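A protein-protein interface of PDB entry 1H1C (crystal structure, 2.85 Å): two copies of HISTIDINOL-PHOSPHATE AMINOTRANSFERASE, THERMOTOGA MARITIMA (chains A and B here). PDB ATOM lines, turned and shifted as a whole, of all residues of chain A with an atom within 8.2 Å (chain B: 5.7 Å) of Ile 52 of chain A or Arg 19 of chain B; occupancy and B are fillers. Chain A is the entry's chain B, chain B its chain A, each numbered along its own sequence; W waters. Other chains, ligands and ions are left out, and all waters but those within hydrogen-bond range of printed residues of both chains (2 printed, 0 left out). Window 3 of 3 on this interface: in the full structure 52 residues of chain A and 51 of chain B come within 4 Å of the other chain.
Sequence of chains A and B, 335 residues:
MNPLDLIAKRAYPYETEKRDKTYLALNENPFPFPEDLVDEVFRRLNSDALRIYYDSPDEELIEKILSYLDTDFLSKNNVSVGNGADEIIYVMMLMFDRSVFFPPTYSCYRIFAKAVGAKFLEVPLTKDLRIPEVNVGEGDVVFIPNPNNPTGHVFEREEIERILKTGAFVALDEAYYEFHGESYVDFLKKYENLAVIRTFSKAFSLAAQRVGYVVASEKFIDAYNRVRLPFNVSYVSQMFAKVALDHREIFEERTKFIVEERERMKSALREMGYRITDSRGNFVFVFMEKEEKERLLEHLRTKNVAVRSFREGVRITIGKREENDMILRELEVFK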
ATOM      1  N   ASN A  46       0.293   9.515 -16.820  1.00  0.00           N
ATOM      2  CA  ASN A  46       0.325   8.859 -15.525  1.00  0.00           C
ATOM      3  C   ASN A  46       1.189   9.617 -14.541  1.00  0.00           C
ATOM      4  O   ASN A  46       2.401   9.696 -14.681  1.00  0.00           O
ATOM      5  CB  ASN A  46       0.819   7.414 -15.700  1.00  0.00           C
ATOM      6  CG  ASN A  46       1.179   6.747 -14.393  1.00  0.00           C
ATOM      7  OD1 ASN A  46       0.612   7.043 -13.342  1.00  0.00           O
ATOM      8  ND2 ASN A  46       2.123   5.822 -14.457  1.00  0.00           N
ATOM      9  N   SER A  47       0.539  10.190 -13.547  1.00  0.00           N
ATOM     10  CA  SER A  47       1.211  10.948 -12.522  1.00  0.00           C
ATOM     11  C   SER A  47       2.452  10.208 -12.004  1.00  0.00           C
ATOM     12  O   SER A  47       3.466  10.823 -11.662  1.00  0.00           O
ATOM     13  CB  SER A  47       0.217  11.200 -11.389  1.00  0.00           C
ATOM     14  OG  SER A  47       0.773  12.015 -10.383  1.00  0.00           O
ATOM     15  N   ASP A  48       2.378   8.881 -11.968  1.00  0.00           N
ATOM     16  CA  ASP A  48       3.485   8.064 -11.456  1.00  0.00           C
ATOM     17  C   ASP A  48       4.693   8.046 -12.377  1.00  0.00           C
ATOM     18  O   ASP A  48       5.764   7.563 -12.010  1.00  0.00           O
ATOM     19  CB  ASP A  48       3.020   6.625 -11.232  1.00  0.00           C
ATOM     20  CG  ASP A  48       3.991   5.825 -10.374  1.00  0.00           C
ATOM     21  OD1 ASP A  48       4.080   4.601 -10.619  1.00  0.00           O
ATOM     22  OD2 ASP A  48       4.650   6.393  -9.457  1.00  0.00           O
ATOM     23  N   ALA A  49       4.513   8.580 -13.574  1.00  0.00           N
ATOM     24  CA  ALA A  49       5.565   8.598 -14.559  1.00  0.00           C
ATOM     25  C   ALA A  49       6.421   9.830 -14.407  1.00  0.00           C
ATOM     26  O   ALA A  49       7.623   9.785 -14.677  1.00  0.00           O
ATOM     27  CB  ALA A  49       4.964   8.544 -15.944  1.00  0.00           C
ATOM     28  N   LEU A  50       5.807  10.920 -13.957  1.00  0.00           N
ATOM     29  CA  LEU A  50       6.513  12.192 -13.788  1.00  0.00           C
ATOM     30  C   LEU A  50       7.709  12.184 -12.824  1.00  0.00           C
ATOM     31  O   LEU A  50       8.585  13.057 -12.902  1.00  0.00           O
ATOM     32  CB  LEU A  50       5.517  13.286 -13.370  1.00  0.00           C
ATOM     33  CG  LEU A  50       4.461  13.634 -14.432  1.00  0.00           C
ATOM     34  CD1 LEU A  50       3.388  14.503 -13.832  1.00  0.00           C
ATOM     35  CD2 LEU A  50       5.105  14.341 -15.618  1.00  0.00           C
ATOM     36  N   ARG A  51       7.753  11.205 -11.926  1.00  0.00           N
ATOM     37  CA  ARG A  51       8.835  11.105 -10.950  1.00  0.00           C
ATOM     38  C   ARG A  51      10.093  10.450 -11.490  1.00  0.00           C
ATOM     39  O   ARG A  51      11.195  10.706 -10.991  1.00  0.00           O
ATOM     40  CB  ARG A  51       8.362  10.320  -9.721  1.00  0.00           C
ATOM     41  CG  ARG A  51       7.694   8.986 -10.034  1.00  0.00           C
ATOM     42  CD  ARG A  51       7.293   8.273  -8.755  1.00  0.00           C
ATOM     43  NE  ARG A  51       8.316   7.321  -8.345  1.00  0.00           N
ATOM     44  CZ  ARG A  51       8.443   6.094  -8.848  1.00  0.00           C
ATOM     45  NH1 ARG A  51       7.600   5.670  -9.779  1.00  0.00           N
ATOM     46  NH2 ARG A  51       9.417   5.295  -8.428  1.00  0.00           N
ATOM     47  N   ILE A  52       9.929   9.604 -12.507  1.00  0.00           N
ATOM     48  CA  ILE A  52      11.056   8.877 -13.083  1.00  0.00           C
ATOM     49  C   ILE A  52      11.609   9.476 -14.362  1.00  0.00           C
ATOM     50  O   ILE A  52      10.988  10.338 -14.971  1.00  0.00           O
ATOM     51  CB  ILE A  52      10.685   7.419 -13.370  1.00  0.00           C
ATOM     52  CG1 ILE A  52       9.617   7.362 -14.459  1.00  0.00           C
ATOM     53  CG2 ILE A  52      10.204   6.764 -12.095  1.00  0.00           C
ATOM     54  CD1 ILE A  52       9.853   6.237 -15.476  1.00  0.00           C
ATOM     55  N   TYR A  53      12.791   9.001 -14.743  1.00  0.00           N
ATOM     56  CA  TYR A  53      13.461   9.445 -15.942  1.00  0.00           C
ATOM     57  C   TYR A  53      12.891   8.689 -17.123  1.00  0.00           C
ATOM     58  O   TYR A  53      13.417   7.667 -17.538  1.00  0.00           O
ATOM     59  CB  TYR A  53      14.953   9.188 -15.817  1.00  0.00           C
ATOM     60  CG  TYR A  53      15.651  10.211 -14.971  1.00  0.00           C
ATOM     61  CD1 TYR A  53      16.101  11.402 -15.526  1.00  0.00           C
ATOM     62  CD2 TYR A  53      15.836  10.013 -13.607  1.00  0.00           C
ATOM     63  CE1 TYR A  53      16.724  12.383 -14.748  1.00  0.00           C
ATOM     64  CE2 TYR A  53      16.462  10.984 -12.819  1.00  0.00           C
ATOM     65  CZ  TYR A  53      16.906  12.165 -13.401  1.00  0.00           C
ATOM     66  OH  TYR A  53      17.561  13.108 -12.645  1.00  0.00           O
ATOM     67  N   TYR A  54      11.800   9.206 -17.659  1.00  0.00           N
ATOM     68  CA  TYR A  54      11.111   8.615 -18.793  1.00  0.00           C
ATOM     69  C   TYR A  54      12.019   8.544 -20.027  1.00  0.00           C
ATOM     70  O   TYR A  54      12.785   9.471 -20.286  1.00  0.00           O
ATOM     71  CB  TYR A  54       9.888   9.470 -19.093  1.00  0.00           C
ATOM     72  CG  TYR A  54       8.843   8.792 -19.909  1.00  0.00           C
ATOM     73  CD1 TYR A  54       8.085   7.763 -19.376  1.00  0.00           C
ATOM     74  CD2 TYR A  54       8.588   9.196 -21.209  1.00  0.00           C
ATOM     75  CE1 TYR A  54       7.090   7.153 -20.124  1.00  0.00           C
ATOM     76  CE2 TYR A  54       7.595   8.597 -21.964  1.00  0.00           C
ATOM     77  CZ  TYR A  54       6.845   7.575 -21.421  1.00  0.00           C
ATOM     78  OH  TYR A  54       5.844   6.987 -22.172  1.00  0.00           O
ATOM     79  N   ASP A  55      11.929   7.447 -20.782  1.00  0.00           N
ATOM     80  CA  ASP A  55      12.727   7.252 -22.006  1.00  0.00           C
ATOM     81  C   ASP A  55      12.557   8.438 -22.949  1.00  0.00           C
ATOM     82  O   ASP A  55      11.430   8.867 -23.206  1.00  0.00           O
ATOM     83  CB  ASP A  55      12.268   6.008 -22.756  1.00  0.00           C
ATOM     84  CG  ASP A  55      12.491   4.729 -21.981  1.00  0.00           C
ATOM     85  OD1 ASP A  55      11.871   3.716 -22.360  1.00  0.00           O
ATOM     86  OD2 ASP A  55      13.279   4.721 -21.010  1.00  0.00           O
ATOM     87  N   PHE A 231      17.865  12.139 -21.764  1.00  0.00           N
ATOM     88  CA  PHE A 231      16.454  12.491 -21.656  1.00  0.00           C
ATOM     89  C   PHE A 231      16.207  13.912 -22.068  1.00  0.00           C
ATOM     90  O   PHE A 231      16.013  14.785 -21.218  1.00  0.00           O
ATOM     91  CB  PHE A 231      16.019  12.300 -20.214  1.00  0.00           C
ATOM     92  CG  PHE A 231      16.511  11.031 -19.639  1.00  0.00           C
ATOM     93  CD1 PHE A 231      17.542  11.026 -18.721  1.00  0.00           C
ATOM     94  CD2 PHE A 231      16.047   9.814 -20.135  1.00  0.00           C
ATOM     95  CE1 PHE A 231      18.117   9.813 -18.313  1.00  0.00           C
ATOM     96  CE2 PHE A 231      16.618   8.610 -19.730  1.00  0.00           C
ATOM     97  CZ  PHE A 231      17.657   8.613 -18.821  1.00  0.00           C
ATOM     98  N   TYR A 235       8.343  13.961 -20.585  1.00  0.00           N
ATOM     99  CA  TYR A 235       7.281  12.975 -20.694  1.00  0.00           C
ATOM    100  C   TYR A 235       6.128  13.693 -21.357  1.00  0.00           C
ATOM    101  O   TYR A 235       5.783  13.414 -22.508  1.00  0.00           O
ATOM    102  CB  TYR A 235       6.869  12.509 -19.299  1.00  0.00           C
ATOM    103  CG  TYR A 235       5.642  11.630 -19.233  1.00  0.00           C
ATOM    104  CD1 TYR A 235       5.618  10.391 -19.854  1.00  0.00           C
ATOM    105  CD2 TYR A 235       4.522  12.017 -18.486  1.00  0.00           C
ATOM    106  CE1 TYR A 235       4.515   9.553 -19.732  1.00  0.00           C
ATOM    107  CE2 TYR A 235       3.413  11.186 -18.350  1.00  0.00           C
ATOM    108  CZ  TYR A 235       3.414   9.954 -18.977  1.00  0.00           C
ATOM    109  OH  TYR A 235       2.319   9.117 -18.869  1.00  0.00           O
ATOM    110  N   GLU B  17      17.520   2.367 -19.435  1.00  0.00           N
ATOM    111  CA  GLU B  17      17.484   1.569 -18.213  1.00  0.00           C
ATOM    112  C   GLU B  17      16.345   0.555 -18.194  1.00  0.00           C
ATOM    113  O   GLU B  17      15.189   0.928 -18.372  1.00  0.00           O
ATOM    114  CB  GLU B  17      17.335   2.484 -16.989  1.00  0.00           C
ATOM    115  CG  GLU B  17      18.599   3.189 -16.581  1.00  0.00           C
ATOM    116  CD  GLU B  17      19.636   2.223 -16.059  1.00  0.00           C
ATOM    117  OE1 GLU B  17      20.832   2.609 -15.996  1.00  0.00           O
ATOM    118  OE2 GLU B  17      19.244   1.082 -15.713  1.00  0.00           O
ATOM    119  N   LYS B  18      16.666  -0.721 -17.991  1.00  0.00           N
ATOM    120  CA  LYS B  18      15.626  -1.743 -17.890  1.00  0.00           C
ATOM    121  C   LYS B  18      15.188  -1.686 -16.423  1.00  0.00           C
ATOM    122  O   LYS B  18      15.961  -2.019 -15.525  1.00  0.00           O
ATOM    123  CB  LYS B  18      16.173  -3.127 -18.274  1.00  0.00           C
ATOM    124  CG  LYS B  18      16.296  -3.323 -19.795  1.00  0.00           C
ATOM    125  CD  LYS B  18      16.757  -4.731 -20.201  1.00  0.00           C
ATOM    126  CE  LYS B  18      16.810  -4.868 -21.730  1.00  0.00           C
ATOM    127  NZ  LYS B  18      17.543  -6.069 -22.234  1.00  0.00           N
ATOM    128  N   ARG B  19      13.950  -1.245 -16.194  1.00  0.00           N
ATOM    129  CA  ARG B  19      13.429  -1.063 -14.840  1.00  0.00           C
ATOM    130  C   ARG B  19      12.763  -2.282 -14.242  1.00  0.00           C
ATOM    131  O   ARG B  19      11.743  -2.742 -14.745  1.00  0.00           O
ATOM    132  CB  ARG B  19      12.455   0.121 -14.824  1.00  0.00           C
ATOM    133  CG  ARG B  19      12.990   1.351 -15.569  1.00  0.00           C
ATOM    134  CD  ARG B  19      12.019   2.528 -15.530  1.00  0.00           C
ATOM    135  NE  ARG B  19      11.885   3.052 -14.175  1.00  0.00           N
ATOM    136  CZ  ARG B  19      12.667   3.985 -13.646  1.00  0.00           C
ATOM    137  NH1 ARG B  19      13.652   4.532 -14.348  1.00  0.00           N
ATOM    138  NH2 ARG B  19      12.474   4.347 -12.394  1.00  0.00           N
ATOM    139  N   ASP B  20      13.353  -2.793 -13.158  1.00  0.00           N
ATOM    140  CA  ASP B  20      12.847  -3.970 -12.447  1.00  0.00           C
ATOM    141  C   ASP B  20      11.562  -3.694 -11.677  1.00  0.00           C
ATOM    142  O   ASP B  20      11.080  -2.559 -11.638  1.00  0.00           O
ATOM    143  CB  ASP B  20      13.903  -4.499 -11.473  1.00  0.00           C
ATOM    144  CG  ASP B  20      14.754  -5.592 -12.077  1.00  0.00           C
ATOM    145  OD1 ASP B  20      14.171  -6.542 -12.640  1.00  0.00           O
ATOM    146  OD2 ASP B  20      15.998  -5.516 -11.988  1.00  0.00           O
ATOM    147  N   LYS B  21      11.016  -4.740 -11.060  1.00  0.00           N
ATOM    148  CA  LYS B  21       9.775  -4.610 -10.302  1.00  0.00           C
ATOM    149  C   LYS B  21       9.958  -3.594  -9.185  1.00  0.00           C
ATOM    150  O   LYS B  21       9.005  -2.928  -8.772  1.00  0.00           O
ATOM    151  CB  LYS B  21       9.356  -5.952  -9.713  1.00  0.00           C
ATOM    152  CG  LYS B  21       8.015  -6.469 -10.219  1.00  0.00           C
ATOM    153  CD  LYS B  21       8.145  -7.322 -11.480  1.00  0.00           C
ATOM    154  CE  LYS B  21       6.867  -8.135 -11.710  1.00  0.00           C
ATOM    155  NZ  LYS B  21       6.934  -9.070 -12.868  1.00  0.00           N
ATOM    156  N   TYR B  23      12.856  -0.679  -8.474  1.00  0.00           N
ATOM    157  CA  TYR B  23      14.022   0.049  -8.949  1.00  0.00           C
ATOM    158  C   TYR B  23      14.539   1.071  -7.932  1.00  0.00           C
ATOM    159  O   TYR B  23      13.826   1.989  -7.517  1.00  0.00           O
ATOM    160  CB  TYR B  23      13.639   0.735 -10.258  1.00  0.00           C
ATOM    161  CG  TYR B  23      14.775   1.250 -11.096  1.00  0.00           C
ATOM    162  CD1 TYR B  23      15.710   0.385 -11.650  1.00  0.00           C
ATOM    163  CD2 TYR B  23      14.899   2.607 -11.359  1.00  0.00           C
ATOM    164  CE1 TYR B  23      16.747   0.864 -12.454  1.00  0.00           C
ATOM    165  CE2 TYR B  23      15.925   3.095 -12.154  1.00  0.00           C
ATOM    166  CZ  TYR B  23      16.849   2.227 -12.702  1.00  0.00           C
ATOM    167  OH  TYR B  23      17.867   2.735 -13.486  1.00  0.00           O
ATOM    168  N   LEU B  26      18.337   4.927  -9.625  1.00  0.00           N
ATOM    169  CA  LEU B  26      18.490   6.269 -10.175  1.00  0.00           C
ATOM    170  C   LEU B  26      18.126   7.472  -9.300  1.00  0.00           C
ATOM    171  O   LEU B  26      17.898   8.567  -9.831  1.00  0.00           O
ATOM    172  CB  LEU B  26      17.712   6.384 -11.491  1.00  0.00           C
ATOM    173  CG  LEU B  26      18.270   5.803 -12.789  1.00  0.00           C
ATOM    174  CD1 LEU B  26      17.387   6.266 -13.952  1.00  0.00           C
ATOM    175  CD2 LEU B  26      19.689   6.270 -13.014  1.00  0.00           C
ATOM    176  N   GLU B  28      15.421   8.357  -7.825  1.00  0.00           N
ATOM    177  CA  GLU B  28      14.159   8.956  -8.206  1.00  0.00           C
ATOM    178  C   GLU B  28      13.281   9.046  -6.963  1.00  0.00           C
ATOM    179  O   GLU B  28      13.313   8.168  -6.100  1.00  0.00           O
ATOM    180  CB  GLU B  28      13.495   8.092  -9.277  1.00  0.00           C
ATOM    181  CG  GLU B  28      14.295   8.020 -10.590  1.00  0.00           C
ATOM    182  CD  GLU B  28      13.911   6.843 -11.485  1.00  0.00           C
ATOM    183  OE1 GLU B  28      14.055   5.689 -11.017  1.00  0.00           O
ATOM    184  OE2 GLU B  28      13.483   7.071 -12.643  1.00  0.00           O
ATOM    185  N   ASN B  29      12.519  10.124  -6.860  1.00  0.00           N
ATOM    186  CA  ASN B  29      11.616  10.309  -5.732  1.00  0.00           C
ATOM    187  C   ASN B  29      10.664   9.114  -5.767  1.00  0.00           C
ATOM    188  O   ASN B  29      10.143   8.777  -6.823  1.00  0.00           O
ATOM    189  CB  ASN B  29      10.829  11.607  -5.913  1.00  0.00           C
ATOM    190  CG  ASN B  29      10.244  12.113  -4.629  1.00  0.00           C
ATOM    191  OD1 ASN B  29       9.478  11.411  -3.962  1.00  0.00           O
ATOM    192  ND2 ASN B  29      10.597  13.345  -4.266  1.00  0.00           N
ATOM    193  N   ALA B 207      11.291  14.587 -12.414  1.00  0.00           N
ATOM    194  CA  ALA B 207      12.425  14.190 -13.264  1.00  0.00           C
ATOM    195  C   ALA B 207      12.022  13.958 -14.726  1.00  0.00           C
ATOM    196  O   ALA B 207      12.818  14.143 -15.651  1.00  0.00           O
ATOM    197  CB  ALA B 207      13.087  12.931 -12.692  1.00  0.00           C
ATOM    198  N   ALA B 208      10.777  13.554 -14.921  1.00  0.00           N
ATOM    199  CA  ALA B 208      10.238  13.287 -16.248  1.00  0.00           C
ATOM    200  C   ALA B 208      10.008  14.565 -17.045  1.00  0.00           C
ATOM    201  O   ALA B 208       9.773  14.519 -18.264  1.00  0.00           O
ATOM    202  CB  ALA B 208       8.913  12.541 -16.108  1.00  0.00           C
ATOM    203  N   GLN B 209      10.054  15.702 -16.356  1.00  0.00           N
ATOM    204  CA  GLN B 209       9.798  16.967 -17.011  1.00  0.00           C
ATOM    205  C   GLN B 209      11.018  17.840 -17.196  1.00  0.00           C
ATOM    206  O   GLN B 209      10.922  18.993 -17.611  1.00  0.00           O
ATOM    207  CB  GLN B 209       8.697  17.693 -16.265  1.00  0.00           C
ATOM    208  CG  GLN B 209       7.355  16.996 -16.454  1.00  0.00           C
ATOM    209  CD  GLN B 209       7.001  16.827 -17.919  1.00  0.00           C
ATOM    210  OE1 GLN B 209       6.920  17.797 -18.655  1.00  0.00           O
ATOM    211  NE2 GLN B 209       6.795  15.594 -18.345  1.00  0.00           N
HETATM  212  O   HOH W   1      12.961  12.141 -17.714  1.00  0.00           O
HETATM  213  O   HOH W   2      12.003  11.895  -8.616  1.00  0.00           O
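The backbone NH (N) of Ala 208 of chain B sits at hydrogen-bond distance from the backbone carbonyl oxygen (O) of Ile 52 of chain A. The backbone carbonyl oxygen (O) of Leu 50 of chain A lies within hydrogen-bond range of the backbone NH (N) of Ala 207 of chain B, at 3.1 Å. The guanidinium group of Arg 51 of chain A is in hydrogen-bond range of the backbone carbonyl oxygen of Asn 29 of chain B (2.8 Å). The backbone NH (N) of Tyr 53 of chain A lies within hydrogen-bond range of the side-chain carboxylate (OE2) of Glu 28 of chain B (2.9 Å). N of Tyr 235 of chain A is in hydrogen-bond range of O of Ala 208 of chain B, 2.8 Å away. The backbone NH (N) of Ala 208 of chain B sits at hydrogen-bond distance from the backbone carbonyl oxygen (O) of Leu 50 of chain A, 3.0 Å away. N of Tyr 235 of chain A lies close to NE2 of Gln 209 of chain B (3.2 Å).
OD2 of Asp 48 of chain A is in salt-bridge range of NH1 of Arg 51 of chain A (3.1 Å). The backbone NH of Asn 46 of chain A sits at hydrogen-bond distance from the side-chain hydroxyl of Tyr 235 of chain A (2.9 Å). The guanidinium group of Arg 19 of chain B is in salt-bridge range of the side-chain carboxylate of Glu 28 of chain B (2.5 Å).
Among the printed residues, merely in contact across the chains: Ile 52 of chain A with Glu 28 of chain B, Ile 52 of chain A with Arg 19 of chain B, Ala 49 of chain A with Ala 208 of chain B, Arg 51 of chain A with Ala 207 of chain B, Leu 50 of chain A with Gln 209 of chain B, Ile 52 of chain A with Ala 207 of chain B, Arg 51 of chain A with Glu 28 of chain B and Tyr 53 of chain A with Ala 207 of chain B.
Ile 52 of chain A touches just these residues of chain B: Arg 19, Glu 28, Ala 207 and Ala 208. Of the printed residues of chain A, Arg 19 of chain B touches Ile 52. Of the printed residues of chain B, Arg 51 of chain A touches Glu 28 (3.9 Å), Asn 29 (2.8 Å) and Ala 207 (3.4 Å). Printed residues of chain B within 4 Å of Leu 50 of chain A: Ala 207 (3.1 Å), Ala 208 (3.0 Å) and Gln 209 (3.4 Å). Printed residues of chain B within 4 Å of Tyr 235 of chain A: Ala 208 (2.8 Å) and Gln 209 (3.2 Å). Lys 18 of chain B touches none of the printed residues of chain A. Tyr 54 of chain A touches none of the printed residues of chain B. The nearest printed residue of chain B that does not touch Ile 52 of chain A is Gln 209 of chain B (5.6 Å). The nearest residue of chain A that does not touch Arg 19 of chain B is Tyr 53 of chain A (4.5 Å).
Of the 12 printed residues of chain A, 6 touch a printed residue of chain B. Hydrophobic or aromatic side chains of chain A within 4 Å of the printed part of chain B: Leu 50, Ile 52, Tyr 53 and Tyr 235.
No position is printed for both chains. Of the 15 pairs that touch across the chains among the printed residues, none has its exchanged pair printed and touching as well.
Water W2 bridges the backbone NH (N) of Asn 29 of chain B (2.5 Å) and the backbone carbonyl oxygen (O) of Arg 51 of chain A (2.8 Å). Water W1 lies within hydrogen-bond range of the backbone carbonyl oxygen (O) of Ala 207 of chain B and the backbone NH (N) of Tyr 54 of chain A.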
